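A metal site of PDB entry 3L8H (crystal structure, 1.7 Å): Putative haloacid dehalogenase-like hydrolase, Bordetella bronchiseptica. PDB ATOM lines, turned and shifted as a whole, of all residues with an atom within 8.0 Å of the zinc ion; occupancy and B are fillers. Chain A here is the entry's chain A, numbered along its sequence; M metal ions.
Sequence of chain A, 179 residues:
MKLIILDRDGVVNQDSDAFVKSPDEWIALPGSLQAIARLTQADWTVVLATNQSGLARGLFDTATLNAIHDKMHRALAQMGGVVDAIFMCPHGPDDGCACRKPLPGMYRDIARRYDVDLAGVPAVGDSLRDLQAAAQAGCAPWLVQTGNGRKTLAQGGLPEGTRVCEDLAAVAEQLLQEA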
ATOM      1  N   THR A  50      16.279 -19.618  -7.838  1.00  0.00           N
ATOM      2  CA  THR A  50      16.470 -20.264  -9.146  1.00  0.00           C
ATOM      3  C   THR A  50      16.492 -19.262 -10.317  1.00  0.00           C
ATOM      4  O   THR A  50      15.652 -18.375 -10.379  1.00  0.00           O
ATOM      5  CB  THR A  50      15.385 -21.359  -9.370  1.00  0.00           C
ATOM      6  OG1 THR A  50      15.491 -21.889 -10.688  1.00  0.00           O
ATOM      7  CG2 THR A  50      13.954 -20.802  -9.165  1.00  0.00           C
ATOM      8  N   ASN A  51      17.454 -19.433 -11.220  1.00  0.00           N
ATOM      9  CA  ASN A  51      17.436 -18.706 -12.496  1.00  0.00           C
ATOM     10  C   ASN A  51      16.428 -19.388 -13.422  1.00  0.00           C
ATOM     11  O   ASN A  51      16.531 -20.591 -13.672  1.00  0.00           O
ATOM     12  CB  ASN A  51      18.825 -18.740 -13.165  1.00  0.00           C
ATOM     13  CG  ASN A  51      19.794 -17.670 -12.633  1.00  0.00           C
ATOM     14  OD1 ASN A  51      19.470 -16.863 -11.762  1.00  0.00           O
ATOM     15  ND2 ASN A  51      21.016 -17.687 -13.162  1.00  0.00           N
ATOM     16  N   GLN A  52      15.465 -18.621 -13.942  1.00  0.00           N
ATOM     17  CA  GLN A  52      14.431 -19.163 -14.840  1.00  0.00           C
ATOM     18  C   GLN A  52      14.314 -18.329 -16.124  1.00  0.00           C
ATOM     19  O   GLN A  52      13.282 -17.719 -16.412  1.00  0.00           O
ATOM     20  CB  GLN A  52      13.079 -19.240 -14.099  1.00  0.00           C
ATOM     21  CG  GLN A  52      13.095 -20.306 -13.025  1.00  0.00           C
ATOM     22  CD  GLN A  52      13.155 -21.693 -13.623  1.00  0.00           C
ATOM     23  OE1 GLN A  52      12.492 -21.961 -14.625  1.00  0.00           O
ATOM     24  NE2 GLN A  52      13.954 -22.586 -13.024  1.00  0.00           N
ATOM     25  N   MET A  88      12.895 -16.329  -7.643  1.00  0.00           N
ATOM     26  CA  MET A  88      13.227 -16.697  -9.023  1.00  0.00           C
ATOM     27  C   MET A  88      13.556 -15.487  -9.840  1.00  0.00           C
ATOM     28  O   MET A  88      12.975 -14.425  -9.644  1.00  0.00           O
ATOM     29  CB  MET A  88      12.119 -17.499  -9.693  1.00  0.00           C
ATOM     30  CG  MET A  88      10.715 -16.976  -9.483  1.00  0.00           C
ATOM     31  SD  MET A  88       9.806 -17.129 -11.192  1.00  0.00           S
ATOM     32  CE  MET A  88      11.234 -16.363 -12.158  1.00  0.00           C
ATOM     33  N   CYS A  89      14.486 -15.677 -10.763  1.00  0.00           N
ATOM     34  CA  CYS A  89      14.895 -14.644 -11.716  1.00  0.00           C
ATOM     35  C   CYS A  89      14.348 -15.034 -13.071  1.00  0.00           C
ATOM     36  O   CYS A  89      14.699 -16.086 -13.601  1.00  0.00           O
ATOM     37  CB  CYS A  89      16.421 -14.615 -11.790  1.00  0.00           C
ATOM     38  SG  CYS A  89      17.003 -13.672 -13.223  1.00  0.00           S
ATOM     39  N   PRO A  90      13.475 -14.185 -13.659  1.00  0.00           N
ATOM     40  CA  PRO A  90      12.819 -14.537 -14.915  1.00  0.00           C
ATOM     41  C   PRO A  90      13.603 -13.996 -16.106  1.00  0.00           C
ATOM     42  O   PRO A  90      13.133 -14.086 -17.234  1.00  0.00           O
ATOM     43  CB  PRO A  90      11.491 -13.792 -14.808  1.00  0.00           C
ATOM     44  CG  PRO A  90      11.892 -12.514 -14.101  1.00  0.00           C
ATOM     45  CD  PRO A  90      12.825 -13.036 -13.012  1.00  0.00           C
ATOM     46  N   HIS A  91      14.780 -13.440 -15.844  1.00  0.00           N
ATOM     47  CA  HIS A  91      15.502 -12.678 -16.878  1.00  0.00           C
ATOM     48  C   HIS A  91      16.499 -13.509 -17.656  1.00  0.00           C
ATOM     49  O   HIS A  91      16.950 -14.561 -17.211  1.00  0.00           O
ATOM     50  CB  HIS A  91      16.227 -11.510 -16.220  1.00  0.00           C
ATOM     51  CG  HIS A  91      15.332 -10.611 -15.444  1.00  0.00           C
ATOM     52  ND1 HIS A  91      15.271 -10.616 -14.065  1.00  0.00           N
ATOM     53  CD2 HIS A  91      14.416  -9.696 -15.864  1.00  0.00           C
ATOM     54  CE1 HIS A  91      14.367  -9.738 -13.666  1.00  0.00           C
ATOM     55  NE2 HIS A  91      13.847  -9.153 -14.735  1.00  0.00           N
ATOM     56  N   GLY A  92      16.871 -13.023 -18.830  1.00  0.00           N
ATOM     57  CA  GLY A  92      17.935 -13.667 -19.583  1.00  0.00           C
ATOM     58  C   GLY A  92      19.311 -13.137 -19.226  1.00  0.00           C
ATOM     59  O   GLY A  92      19.446 -12.176 -18.479  1.00  0.00           O
ATOM     60  N   ASP A  95      20.002  -9.283 -19.707  1.00  0.00           N
ATOM     61  CA  ASP A  95      18.873  -8.429 -19.374  1.00  0.00           C
ATOM     62  C   ASP A  95      19.124  -7.423 -18.252  1.00  0.00           C
ATOM     63  O   ASP A  95      18.212  -6.696 -17.888  1.00  0.00           O
ATOM     64  CB  ASP A  95      17.632  -9.270 -19.054  1.00  0.00           C
ATOM     65  CG  ASP A  95      16.966  -9.817 -20.299  1.00  0.00           C
ATOM     66  OD1 ASP A  95      17.236  -9.296 -21.420  1.00  0.00           O
ATOM     67  OD2 ASP A  95      16.172 -10.756 -20.161  1.00  0.00           O
ATOM     68  N   GLY A  96      20.328  -7.406 -17.696  1.00  0.00           N
ATOM     69  CA  GLY A  96      20.722  -6.348 -16.779  1.00  0.00           C
ATOM     70  C   GLY A  96      20.002  -6.282 -15.443  1.00  0.00           C
ATOM     71  O   GLY A  96      19.928  -5.226 -14.812  1.00  0.00           O
ATOM     72  N   CYS A  97      19.476  -7.412 -14.991  1.00  0.00           N
ATOM     73  CA  CYS A  97      18.751  -7.396 -13.710  1.00  0.00           C
ATOM     74  C   CYS A  97      19.680  -7.522 -12.506  1.00  0.00           C
ATOM     75  O   CYS A  97      20.886  -7.722 -12.643  1.00  0.00           O
ATOM     76  CB  CYS A  97      17.721  -8.520 -13.667  1.00  0.00           C
ATOM     77  SG  CYS A  97      18.471 -10.158 -13.640  1.00  0.00           S
ATOM     78  N   ALA A  98      19.091  -7.429 -11.314  1.00  0.00           N
ATOM     79  CA  ALA A  98      19.849  -7.576 -10.071  1.00  0.00           C
ATOM     80  C   ALA A  98      19.842  -9.032  -9.596  1.00  0.00           C
ATOM     81  O   ALA A  98      20.608  -9.381  -8.706  1.00  0.00           O
ATOM     82  CB  ALA A  98      19.241  -6.701  -8.960  1.00  0.00           C
ATOM     83  N   CYS A  99      18.960  -9.836 -10.163  1.00  0.00           N
ATOM     84  CA  CYS A  99      18.639 -11.125  -9.522  1.00  0.00           C
ATOM     85  C   CYS A  99      19.260 -12.339 -10.212  1.00  0.00           C
ATOM     86  O   CYS A  99      19.234 -13.448  -9.655  1.00  0.00           O
ATOM     87  CB  CYS A  99      17.124 -11.306  -9.390  1.00  0.00           C
ATOM     88  SG  CYS A  99      16.112 -10.622 -10.729  1.00  0.00           S
ATOM     89  N   ARG A 100      19.806 -12.169 -11.402  1.00  0.00           N
ATOM     90  CA  ARG A 100      20.398 -13.310 -12.087  1.00  0.00           C
ATOM     91  C   ARG A 100      21.731 -13.746 -11.492  1.00  0.00           C
ATOM     92  O   ARG A 100      22.723 -13.015 -11.538  1.00  0.00           O
ATOM     93  CB  ARG A 100      20.544 -13.044 -13.579  1.00  0.00           C
ATOM     94  CG  ARG A 100      21.210 -14.197 -14.318  1.00  0.00           C
ATOM     95  CD  ARG A 100      21.122 -14.010 -15.832  1.00  0.00           C
ATOM     96  NE  ARG A 100      22.009 -14.952 -16.516  1.00  0.00           N
ATOM     97  CZ  ARG A 100      21.638 -16.177 -16.891  1.00  0.00           C
ATOM     98  NH1 ARG A 100      22.520 -16.960 -17.504  1.00  0.00           N
ATOM     99  NH2 ARG A 100      20.412 -16.619 -16.648  1.00  0.00           N
ATOM    100  N   LYS A 101      21.791 -14.969 -10.942  1.00  0.00           N
ATOM    101  CA  LYS A 101      23.062 -15.477 -10.456  1.00  0.00           C
ATOM    102  C   LYS A 101      24.069 -15.422 -11.615  1.00  0.00           C
ATOM    103  O   LYS A 101      23.704 -15.763 -12.731  1.00  0.00           O
ATOM    104  CB  LYS A 101      22.897 -16.929  -9.978  1.00  0.00           C
ATOM    105  CG  LYS A 101      21.742 -17.131  -9.002  1.00  0.00           C
ATOM    106  CD  LYS A 101      21.852 -18.539  -8.411  1.00  0.00           C
ATOM    107  CE  LYS A 101      20.574 -19.036  -7.818  1.00  0.00           C
ATOM    108  NZ  LYS A 101      20.852 -20.302  -7.072  1.00  0.00           N
ATOM    109  N   LEU A 103      24.914 -12.734  -9.641  1.00  0.00           N
ATOM    110  CA  LEU A 103      24.606 -11.604  -8.774  1.00  0.00           C
ATOM    111  C   LEU A 103      23.859 -12.118  -7.543  1.00  0.00           C
ATOM    112  O   LEU A 103      23.132 -13.089  -7.635  1.00  0.00           O
ATOM    113  CB  LEU A 103      23.751 -10.583  -9.505  1.00  0.00           C
ATOM    114  CG  LEU A 103      24.447  -9.889 -10.677  1.00  0.00           C
ATOM    115  CD1 LEU A 103      23.444  -9.123 -11.518  1.00  0.00           C
ATOM    116  CD2 LEU A 103      25.548  -8.968 -10.175  1.00  0.00           C
ATOM    117  N   MET A 106      18.912 -12.289  -5.307  1.00  0.00           N
ATOM    118  CA  MET A 106      17.884 -13.171  -4.721  1.00  0.00           C
ATOM    119  C   MET A 106      18.225 -13.532  -3.308  1.00  0.00           C
ATOM    120  O   MET A 106      17.313 -13.649  -2.456  1.00  0.00           O
ATOM    121  CB  MET A 106      17.719 -14.443  -5.554  1.00  0.00           C
ATOM    122  CG  MET A 106      16.978 -14.210  -6.846  1.00  0.00           C
ATOM    123  SD  MET A 106      16.473 -15.887  -7.717  1.00  0.00           S
ATOM    124  CE  MET A 106      18.238 -16.336  -8.494  1.00  0.00           C
HETATM  125 ZN    ZN M   1      16.740 -11.378 -12.802  1.00  0.00          ZN
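The side-chain sulfur (SG) of Cys 97 lies close to the backbone NH (N) of Arg 100. N of Cys 89 sits at hydrogen-bond distance from O of Thr 50 (3.0 Å). The backbone NH (N) of Gln 52 sits at hydrogen-bond distance from the backbone carbonyl oxygen (O) of Cys 89, 2.7 Å away. The side-chain sulfur (SD) of Met 106 lies within hydrogen-bond range of the backbone NH (N) of Cys 89 (3.6 Å). The side-chain sulfur of Cys 89 lies close to the backbone NH of Arg 100, 3.7 Å away.
Arg 100 touches the zinc ion. Within 4 Å of the zinc ion: Cys 89, His 91, Cys 97, Cys 99 and Arg 100. Along chain A the residues within 4 Å of the zinc ion span positions 89 to 100.
The zinc ion is bound by a ring nitrogen (ND1) of His 91, at 2.1 Å. The side-chain sulfur (SG) of Cys 97 is bound to the zinc ion, 2.3 Å away. The zinc ion is bound by SG of Cys 99 (2.3 Å). The zinc ion is bound by SG of Cys 89, at 2.3 Å. The zinc ion has four donor atoms within binding distance.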
